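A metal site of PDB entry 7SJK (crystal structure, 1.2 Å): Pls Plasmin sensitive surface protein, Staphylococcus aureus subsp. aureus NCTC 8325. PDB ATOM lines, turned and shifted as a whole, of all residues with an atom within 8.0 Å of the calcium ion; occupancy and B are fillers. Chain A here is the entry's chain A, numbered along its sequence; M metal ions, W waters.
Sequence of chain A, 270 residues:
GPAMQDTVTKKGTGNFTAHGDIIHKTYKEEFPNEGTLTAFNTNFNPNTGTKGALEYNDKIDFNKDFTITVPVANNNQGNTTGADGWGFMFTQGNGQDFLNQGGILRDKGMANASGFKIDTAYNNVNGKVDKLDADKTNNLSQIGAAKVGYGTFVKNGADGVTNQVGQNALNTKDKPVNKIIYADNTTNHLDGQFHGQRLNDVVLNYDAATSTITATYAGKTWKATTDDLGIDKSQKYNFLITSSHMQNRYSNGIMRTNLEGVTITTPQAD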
ATOM      1  N   ASN A  79      -4.301 -22.121 -21.508  1.00  0.00           N
ATOM      2  CA  ASN A  79      -3.886 -20.731 -21.310  1.00  0.00           C
ATOM      3  C   ASN A  79      -2.413 -20.621 -20.810  1.00  0.00           C
ATOM      4  O   ASN A  79      -1.901 -19.498 -20.796  1.00  0.00           O
ATOM      5  CB  ASN A  79      -4.938 -19.989 -20.493  1.00  0.00           C
ATOM      6  CG  ASN A  79      -5.046 -20.438 -19.052  1.00  0.00           C
ATOM      7  OD1 ASN A  79      -4.167 -21.052 -18.463  1.00  0.00           O
ATOM      8  ND2 ASN A  79      -6.195 -20.129 -18.478  1.00  0.00           N
ATOM      9  N   ALA A  83      -1.224 -18.594 -27.257  1.00  0.00           N
ATOM     10  CA  ALA A  83      -1.015 -17.181 -27.547  1.00  0.00           C
ATOM     11  C   ALA A  83      -1.571 -16.308 -26.450  1.00  0.00           C
ATOM     12  O   ALA A  83      -2.467 -16.700 -25.653  1.00  0.00           O
ATOM     13  CB  ALA A  83      -1.638 -16.796 -28.877  1.00  0.00           C
ATOM     14  N   ASP A  84      -1.090 -15.062 -26.420  1.00  0.00           N
ATOM     15  CA  ASP A  84      -1.510 -14.072 -25.442  1.00  0.00           C
ATOM     16  C   ASP A  84      -2.944 -13.627 -25.664  1.00  0.00           C
ATOM     17  O   ASP A  84      -3.625 -13.231 -24.710  1.00  0.00           O
ATOM     18  CB  ASP A  84      -0.600 -12.854 -25.507  1.00  0.00           C
ATOM     19  CG  ASP A  84       0.823 -13.163 -25.093  1.00  0.00           C
ATOM     20  OD1 ASP A  84       1.029 -14.007 -24.223  1.00  0.00           O
ATOM     21  OD2 ASP A  84       1.736 -12.446 -25.603  1.00  0.00           O
ATOM     22  N   GLY A  85      -3.421 -13.614 -26.913  1.00  0.00           N
ATOM     23  CA  GLY A  85      -4.776 -13.188 -27.228  1.00  0.00           C
ATOM     24  C   GLY A  85      -4.826 -12.234 -28.391  1.00  0.00           C
ATOM     25  O   GLY A  85      -3.910 -12.288 -29.251  1.00  0.00           O
ATOM     26  N   ILE A 104      -1.063  -4.182 -25.700  1.00  0.00           N
ATOM     27  CA  ILE A 104      -2.032  -4.093 -24.590  1.00  0.00           C
ATOM     28  C   ILE A 104      -2.327  -5.485 -24.029  1.00  0.00           C
ATOM     29  O   ILE A 104      -3.344  -5.571 -23.256  1.00  0.00           O
ATOM     30  CB  ILE A 104      -3.293  -3.278 -25.004  1.00  0.00           C
ATOM     31  CG1 ILE A 104      -3.985  -3.945 -26.207  1.00  0.00           C
ATOM     32  CG2 ILE A 104      -2.964  -1.844 -25.227  1.00  0.00           C
ATOM     33  CD1 ILE A 104      -5.390  -3.355 -26.443  1.00  0.00           C
ATOM     34  N   LEU A 105      -1.632  -6.535 -24.388  1.00  0.00           N
ATOM     35  CA  LEU A 105      -1.910  -7.909 -23.970  1.00  0.00           C
ATOM     36  C   LEU A 105      -1.133  -8.405 -22.759  1.00  0.00           C
ATOM     37  O   LEU A 105      -1.337  -9.523 -22.315  1.00  0.00           O
ATOM     38  CB  LEU A 105      -1.702  -8.833 -25.175  1.00  0.00           C
ATOM     39  CG  LEU A 105      -2.854  -8.933 -26.168  1.00  0.00           C
ATOM     40  CD1 LEU A 105      -2.439  -9.648 -27.424  1.00  0.00           C
ATOM     41  CD2 LEU A 105      -4.060  -9.658 -25.541  1.00  0.00           C
ATOM     42  N   ARG A 106      -0.126  -7.616 -22.368  1.00  0.00           N
ATOM     43  CA  ARG A 106       0.807  -8.040 -21.307  1.00  0.00           C
ATOM     44  C   ARG A 106       0.765  -7.046 -20.143  1.00  0.00           C
ATOM     45  O   ARG A 106      -0.302  -6.480 -19.860  1.00  0.00           O
ATOM     46  CB  ARG A 106       2.189  -8.215 -21.938  1.00  0.00           C
ATOM     47  CG  ARG A 106       2.265  -9.349 -22.953  1.00  0.00           C
ATOM     48  CD  ARG A 106       1.961 -10.708 -22.311  1.00  0.00           C
ATOM     49  NE  ARG A 106       2.637 -11.011 -21.053  1.00  0.00           N
ATOM     50  CZ  ARG A 106       3.929 -11.260 -20.942  1.00  0.00           C
ATOM     51  NH1 ARG A 106       4.730 -11.483 -21.968  1.00  0.00           N
ATOM     52  NH2 ARG A 106       4.393 -11.416 -19.724  1.00  0.00           N
ATOM     53  N   ASP A 107       1.875  -6.891 -19.452  1.00  0.00           N
ATOM     54  CA  ASP A 107       1.973  -6.004 -18.271  1.00  0.00           C
ATOM     55  C   ASP A 107       2.184  -4.554 -18.705  1.00  0.00           C
ATOM     56  O   ASP A 107       1.813  -3.630 -17.976  1.00  0.00           O
ATOM     57  CB  ASP A 107       3.097  -6.494 -17.349  1.00  0.00           C
ATOM     58  CG  ASP A 107       4.426  -6.794 -18.046  1.00  0.00           C
ATOM     59  OD1 ASP A 107       4.461  -7.028 -19.302  1.00  0.00           O
ATOM     60  OD2 ASP A 107       5.418  -6.842 -17.353  1.00  0.00           O
ATOM     61  N   LYS A 117      -9.042  -5.969 -25.236  1.00  0.00           N
ATOM     62  CA  LYS A 117      -8.313  -7.198 -25.357  1.00  0.00           C
ATOM     63  C   LYS A 117      -9.188  -8.398 -25.137  1.00  0.00           C
ATOM     64  O   LYS A 117     -10.112  -8.376 -24.260  1.00  0.00           O
ATOM     65  CB  LYS A 117      -7.077  -7.276 -24.449  1.00  0.00           C
ATOM     66  CG  LYS A 117      -7.326  -7.422 -22.971  1.00  0.00           C
ATOM     67  CD  LYS A 117      -6.023  -7.704 -22.203  1.00  0.00           C
ATOM     68  CE  LYS A 117      -6.209  -7.916 -20.745  1.00  0.00           C
ATOM     69  NZ  LYS A 117      -4.999  -8.494 -20.073  1.00  0.00           N
ATOM     70  N   ILE A 118      -8.929  -9.425 -25.901  1.00  0.00           N
ATOM     71  CA  ILE A 118      -9.325 -10.832 -25.636  1.00  0.00           C
ATOM     72  C   ILE A 118      -8.091 -11.533 -25.116  1.00  0.00           C
ATOM     73  O   ILE A 118      -7.169 -11.749 -25.938  1.00  0.00           O
ATOM     74  CB  ILE A 118      -9.921 -11.516 -26.856  1.00  0.00           C
ATOM     75  CG1 ILE A 118     -11.176 -10.802 -27.397  1.00  0.00           C
ATOM     76  CG2 ILE A 118     -10.214 -12.981 -26.557  1.00  0.00           C
ATOM     77  CD1 ILE A 118     -11.583 -11.232 -28.774  1.00  0.00           C
ATOM     78  N   ASP A 119      -7.967 -11.712 -23.854  1.00  0.00           N
ATOM     79  CA  ASP A 119      -6.769 -12.268 -23.201  1.00  0.00           C
ATOM     80  C   ASP A 119      -6.923 -13.769 -23.072  1.00  0.00           C
ATOM     81  O   ASP A 119      -7.881 -14.212 -22.435  1.00  0.00           O
ATOM     82  CB  ASP A 119      -6.544 -11.570 -21.856  1.00  0.00           C
ATOM     83  CG  ASP A 119      -5.174 -11.933 -21.301  1.00  0.00           C
ATOM     84  OD1 ASP A 119      -4.805 -13.102 -21.300  1.00  0.00           O
ATOM     85  OD2 ASP A 119      -4.464 -11.025 -20.758  1.00  0.00           O
ATOM     86  N   THR A 120      -6.072 -14.510 -23.756  1.00  0.00           N
ATOM     87  CA  THR A 120      -6.163 -15.973 -23.811  1.00  0.00           C
ATOM     88  C   THR A 120      -4.997 -16.675 -23.127  1.00  0.00           C
ATOM     89  O   THR A 120      -4.764 -17.843 -23.361  1.00  0.00           O
ATOM     90  CB  THR A 120      -6.300 -16.419 -25.265  1.00  0.00           C
ATOM     91  OG1 THR A 120      -5.147 -16.012 -26.042  1.00  0.00           O
ATOM     92  CG2 THR A 120      -7.500 -15.823 -25.955  1.00  0.00           C
ATOM     93  N   ALA A 121      -4.250 -15.952 -22.286  1.00  0.00           N
ATOM     94  CA  ALA A 121      -3.082 -16.527 -21.636  1.00  0.00           C
ATOM     95  C   ALA A 121      -3.003 -16.153 -20.147  1.00  0.00           C
ATOM     96  O   ALA A 121      -3.201 -14.968 -19.812  1.00  0.00           O
ATOM     97  CB  ALA A 121      -1.819 -16.118 -22.327  1.00  0.00           C
ATOM     98  N   TYR A 122      -2.573 -17.087 -19.346  1.00  0.00           N
ATOM     99  CA  TYR A 122      -2.142 -16.804 -17.962  1.00  0.00           C
ATOM    100  C   TYR A 122      -0.626 -16.638 -18.054  1.00  0.00           C
ATOM    101  O   TYR A 122       0.104 -17.642 -18.243  1.00  0.00           O
ATOM    102  CB  TYR A 122      -2.513 -17.926 -17.019  1.00  0.00           C
ATOM    103  CG  TYR A 122      -2.099 -17.715 -15.607  1.00  0.00           C
ATOM    104  CD1 TYR A 122      -2.901 -16.937 -14.774  1.00  0.00           C
ATOM    105  CD2 TYR A 122      -0.986 -18.328 -15.036  1.00  0.00           C
ATOM    106  CE1 TYR A 122      -2.593 -16.736 -13.443  1.00  0.00           C
ATOM    107  CE2 TYR A 122      -0.707 -18.176 -13.695  1.00  0.00           C
ATOM    108  CZ  TYR A 122      -1.493 -17.361 -12.912  1.00  0.00           C
ATOM    109  OH  TYR A 122      -1.272 -17.242 -11.572  1.00  0.00           O
ATOM    110  N   ASN A 123      -0.170 -15.394 -17.976  1.00  0.00           N
ATOM    111  CA  ASN A 123       1.259 -15.047 -18.272  1.00  0.00           C
ATOM    112  C   ASN A 123       2.044 -14.981 -16.974  1.00  0.00           C
ATOM    113  O   ASN A 123       1.759 -14.094 -16.159  1.00  0.00           O
ATOM    114  CB  ASN A 123       1.346 -13.744 -19.027  1.00  0.00           C
ATOM    115  CG  ASN A 123       0.647 -13.790 -20.373  1.00  0.00           C
ATOM    116  OD1 ASN A 123      -0.574 -13.560 -20.452  1.00  0.00           O
ATOM    117  ND2 ASN A 123       1.365 -14.186 -21.402  1.00  0.00           N
ATOM    118  N   ASN A 124       2.967 -15.881 -16.802  1.00  0.00           N
ATOM    119  CA  ASN A 124       3.757 -16.045 -15.569  1.00  0.00           C
ATOM    120  C   ASN A 124       5.229 -16.158 -15.959  1.00  0.00           C
ATOM    121  O   ASN A 124       5.607 -17.095 -16.622  1.00  0.00           O
ATOM    122  CB  ASN A 124       3.234 -17.268 -14.820  1.00  0.00           C
ATOM    123  CG  ASN A 124       3.935 -17.543 -13.510  1.00  0.00           C
ATOM    124  OD1 ASN A 124       4.851 -16.830 -13.169  1.00  0.00           O
ATOM    125  ND2 ASN A 124       3.518 -18.575 -12.803  1.00  0.00           N
ATOM    126  N   VAL A 129       3.295 -12.970 -12.153  1.00  0.00           N
ATOM    127  CA  VAL A 129       2.102 -13.072 -13.001  1.00  0.00           C
ATOM    128  C   VAL A 129       1.679 -11.702 -13.476  1.00  0.00           C
ATOM    129  O   VAL A 129       1.622 -10.767 -12.666  1.00  0.00           O
ATOM    130  CB  VAL A 129       0.995 -13.815 -12.239  1.00  0.00           C
ATOM    131  CG1 VAL A 129      -0.294 -13.873 -13.055  1.00  0.00           C
ATOM    132  CG2 VAL A 129       1.424 -15.204 -11.843  1.00  0.00           C
ATOM    133  N   ASP A 130       1.356 -11.587 -14.752  1.00  0.00           N
ATOM    134  CA  ASP A 130       0.811 -10.339 -15.244  1.00  0.00           C
ATOM    135  C   ASP A 130      -0.349  -9.951 -14.344  1.00  0.00           C
ATOM    136  O   ASP A 130      -1.242 -10.739 -14.018  1.00  0.00           O
ATOM    137  CB  ASP A 130       0.347 -10.382 -16.690  1.00  0.00           C
ATOM    138  CG  ASP A 130       1.436 -10.477 -17.749  1.00  0.00           C
ATOM    139  OD1 ASP A 130       2.663 -10.528 -17.438  1.00  0.00           O
ATOM    140  OD2 ASP A 130       1.011 -10.431 -18.957  1.00  0.00           O
ATOM    141  N   LYS A 131      -0.436  -8.670 -14.034  1.00  0.00           N
ATOM    142  CA  LYS A 131      -1.311  -8.172 -13.014  1.00  0.00           C
ATOM    143  C   LYS A 131      -2.768  -8.465 -13.323  1.00  0.00           C
ATOM    144  O   LYS A 131      -3.501  -8.962 -12.419  1.00  0.00           O
ATOM    145  CB  LYS A 131      -1.080  -6.659 -12.853  1.00  0.00           C
ATOM    146  CG  LYS A 131      -1.862  -6.054 -11.730  1.00  0.00           C
ATOM    147  CD  LYS A 131      -1.435  -4.668 -11.475  1.00  0.00           C
ATOM    148  CE  LYS A 131      -1.960  -3.723 -12.542  1.00  0.00           C
ATOM    149  NZ  LYS A 131      -1.701  -2.333 -12.069  1.00  0.00           N
ATOM    150  N   LEU A 132      -3.218  -8.149 -14.526  1.00  0.00           N
ATOM    151  CA  LEU A 132      -4.658  -8.361 -14.831  1.00  0.00           C
ATOM    152  C   LEU A 132      -4.996  -9.868 -14.812  1.00  0.00           C
ATOM    153  O   LEU A 132      -6.122 -10.233 -14.448  1.00  0.00           O
ATOM    154  CB  LEU A 132      -5.046  -7.689 -16.152  1.00  0.00           C
ATOM    155  CG  LEU A 132      -5.384  -6.196 -16.085  1.00  0.00           C
ATOM    156  CD1 LEU A 132      -4.193  -5.373 -15.568  1.00  0.00           C
ATOM    157  CD2 LEU A 132      -5.889  -5.700 -17.442  1.00  0.00           C
ATOM    158  N   ASP A 133      -4.075 -10.715 -15.208  1.00  0.00           N
ATOM    159  CA  ASP A 133      -4.270 -12.169 -15.184  1.00  0.00           C
ATOM    160  C   ASP A 133      -4.456 -12.688 -13.759  1.00  0.00           C
ATOM    161  O   ASP A 133      -4.974 -13.794 -13.609  1.00  0.00           O
ATOM    162  CB  ASP A 133      -3.068 -12.881 -15.823  1.00  0.00           C
ATOM    163  CG  ASP A 133      -2.949 -12.693 -17.302  1.00  0.00           C
ATOM    164  OD1 ASP A 133      -3.851 -12.193 -18.014  1.00  0.00           O
ATOM    165  OD2 ASP A 133      -1.839 -13.071 -17.847  1.00  0.00           O
ATOM    166  N   ALA A 134      -3.930 -11.992 -12.770  1.00  0.00           N
ATOM    167  CA  ALA A 134      -3.931 -12.403 -11.369  1.00  0.00           C
ATOM    168  C   ALA A 134      -5.246 -11.997 -10.689  1.00  0.00           C
ATOM    169  O   ALA A 134      -5.413 -12.342  -9.509  1.00  0.00           O
ATOM    170  CB  ALA A 134      -2.740 -11.855 -10.642  1.00  0.00           C
ATOM    171  N   LEU A 140      -9.949 -14.054 -14.128  1.00  0.00           N
ATOM    172  CA  LEU A 140      -9.367 -15.353 -14.444  1.00  0.00           C
ATOM    173  C   LEU A 140      -9.068 -16.170 -13.208  1.00  0.00           C
ATOM    174  O   LEU A 140      -8.344 -15.713 -12.352  1.00  0.00           O
ATOM    175  CB  LEU A 140      -8.127 -15.190 -15.303  1.00  0.00           C
ATOM    176  CG  LEU A 140      -7.425 -16.443 -15.847  1.00  0.00           C
ATOM    177  CD1 LEU A 140      -8.385 -17.251 -16.722  1.00  0.00           C
ATOM    178  CD2 LEU A 140      -6.201 -16.027 -16.660  1.00  0.00           C
ATOM    179  N   GLY A 149      -9.961 -17.593 -20.805  1.00  0.00           N
ATOM    180  CA  GLY A 149      -9.317 -16.274 -20.708  1.00  0.00           C
ATOM    181  C   GLY A 149     -10.382 -15.266 -20.310  1.00  0.00           C
ATOM    182  O   GLY A 149     -11.348 -15.612 -19.582  1.00  0.00           O
ATOM    183  N   TYR A 150     -10.299 -14.037 -20.777  1.00  0.00           N
ATOM    184  CA  TYR A 150     -11.186 -12.973 -20.395  1.00  0.00           C
ATOM    185  C   TYR A 150     -11.134 -11.828 -21.356  1.00  0.00           C
ATOM    186  O   TYR A 150     -10.099 -11.682 -22.050  1.00  0.00           O
ATOM    187  CB  TYR A 150     -10.936 -12.520 -18.955  1.00  0.00           C
ATOM    188  CG  TYR A 150      -9.581 -11.927 -18.710  1.00  0.00           C
ATOM    189  CD1 TYR A 150      -8.499 -12.781 -18.500  1.00  0.00           C
ATOM    190  CD2 TYR A 150      -9.382 -10.577 -18.641  1.00  0.00           C
ATOM    191  CE1 TYR A 150      -7.224 -12.248 -18.240  1.00  0.00           C
ATOM    192  CE2 TYR A 150      -8.120 -10.048 -18.360  1.00  0.00           C
ATOM    193  CZ  TYR A 150      -7.042 -10.895 -18.156  1.00  0.00           C
ATOM    194  OH  TYR A 150      -5.774 -10.337 -17.930  1.00  0.00           O
ATOM    195  N   MET A 246       4.111 -15.828 -26.128  1.00  0.00           N
ATOM    196  CA  MET A 246       5.159 -15.669 -25.114  1.00  0.00           C
ATOM    197  C   MET A 246       6.257 -16.693 -25.381  1.00  0.00           C
ATOM    198  O   MET A 246       6.000 -17.834 -25.876  1.00  0.00           O
ATOM    199  CB  MET A 246       4.522 -15.809 -23.733  1.00  0.00           C
ATOM    200  CG  MET A 246       5.408 -15.440 -22.594  1.00  0.00           C
ATOM    201  SD  MET A 246       4.435 -15.687 -21.121  1.00  0.00           S
ATOM    202  CE  MET A 246       5.719 -15.198 -19.961  1.00  0.00           C
ATOM    203  N   ARG A 249       7.051 -21.252 -24.385  1.00  0.00           N
ATOM    204  CA  ARG A 249       5.830 -22.042 -24.653  1.00  0.00           C
ATOM    205  C   ARG A 249       6.091 -22.903 -25.884  1.00  0.00           C
ATOM    206  O   ARG A 249       6.536 -22.382 -26.894  1.00  0.00           O
ATOM    207  CB  ARG A 249       4.635 -21.092 -24.875  1.00  0.00           C
ATOM    208  CG  ARG A 249       4.289 -20.336 -23.615  1.00  0.00           C
ATOM    209  CD  ARG A 249       3.078 -19.424 -23.703  1.00  0.00           C
ATOM    210  NE  ARG A 249       2.789 -18.867 -22.381  1.00  0.00           N
ATOM    211  CZ  ARG A 249       1.564 -18.793 -21.824  1.00  0.00           C
ATOM    212  NH1 ARG A 249       0.476 -19.035 -22.536  1.00  0.00           N
ATOM    213  NH2 ARG A 249       1.453 -18.384 -20.578  1.00  0.00           N
HETATM  214 CA    CA M   1      -2.701 -12.667 -20.147  1.00  0.00          CA
HETATM  215  O   HOH W   1      -1.502 -10.598 -19.854  1.00  0.00           O
HETATM  216  O   HOH W   2      -2.189 -12.157 -22.485  1.00  0.00           O
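O of Asn 123 is in hydrogen-bond range of N of Asp 130, 2.9 Å away. The guanidinium group (NE) of Arg 106 sits close to the side-chain amide nitrogen (ND2) of Asn 123. ND2 of Asn 123 lies within hydrogen-bond range of SD of Met 246 (3.4 Å). The side-chain carboxylate (OD1) of Asp 84 lies within hydrogen-bond range of the side-chain amide nitrogen (ND2) of Asn 123. N of Asp 133 sits at hydrogen-bond distance from OH of Tyr 150, 3.2 Å away. The backbone NH of Asp 119 is in hydrogen-bond range of the backbone carbonyl oxygen of Tyr 150. OD2 of Asp 119 sits close to NZ of Lys 117 (2.7 Å).
The calcium ion is bound by the side-chain amide oxygen (OD1) of Asn 123 (2.3 Å), the backbone carbonyl oxygen (O) of Ala 121 (2.4 Å), water W1 (2.4 Å), the side-chain carboxylate (OD1) of Asp 119 (2.4 Å), water W2 (2.4 Å), the side-chain carboxylate (OD1) of Asp 133 (2.5 Å), the side-chain carboxylate (OD2) of Asp 119 (2.5 Å) and the side-chain carboxylate (OD2) of Asp 133 (2.5 Å). The calcium ion has eight donor atoms within binding distance.
Of the 27 residues printed, 4 come within 4 Å of the calcium ion.
Water W2 lies within hydrogen-bond range of the backbone carbonyl oxygen (O) of Leu 105 (2.8 Å) and the backbone carbonyl oxygen (O) of Asp 84 (2.9 Å). Water W1 lies within hydrogen-bond range of the side-chain carboxylate of Asp 130 (2.7 Å) and the backbone carbonyl oxygen of Leu 105 (2.7 Å).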
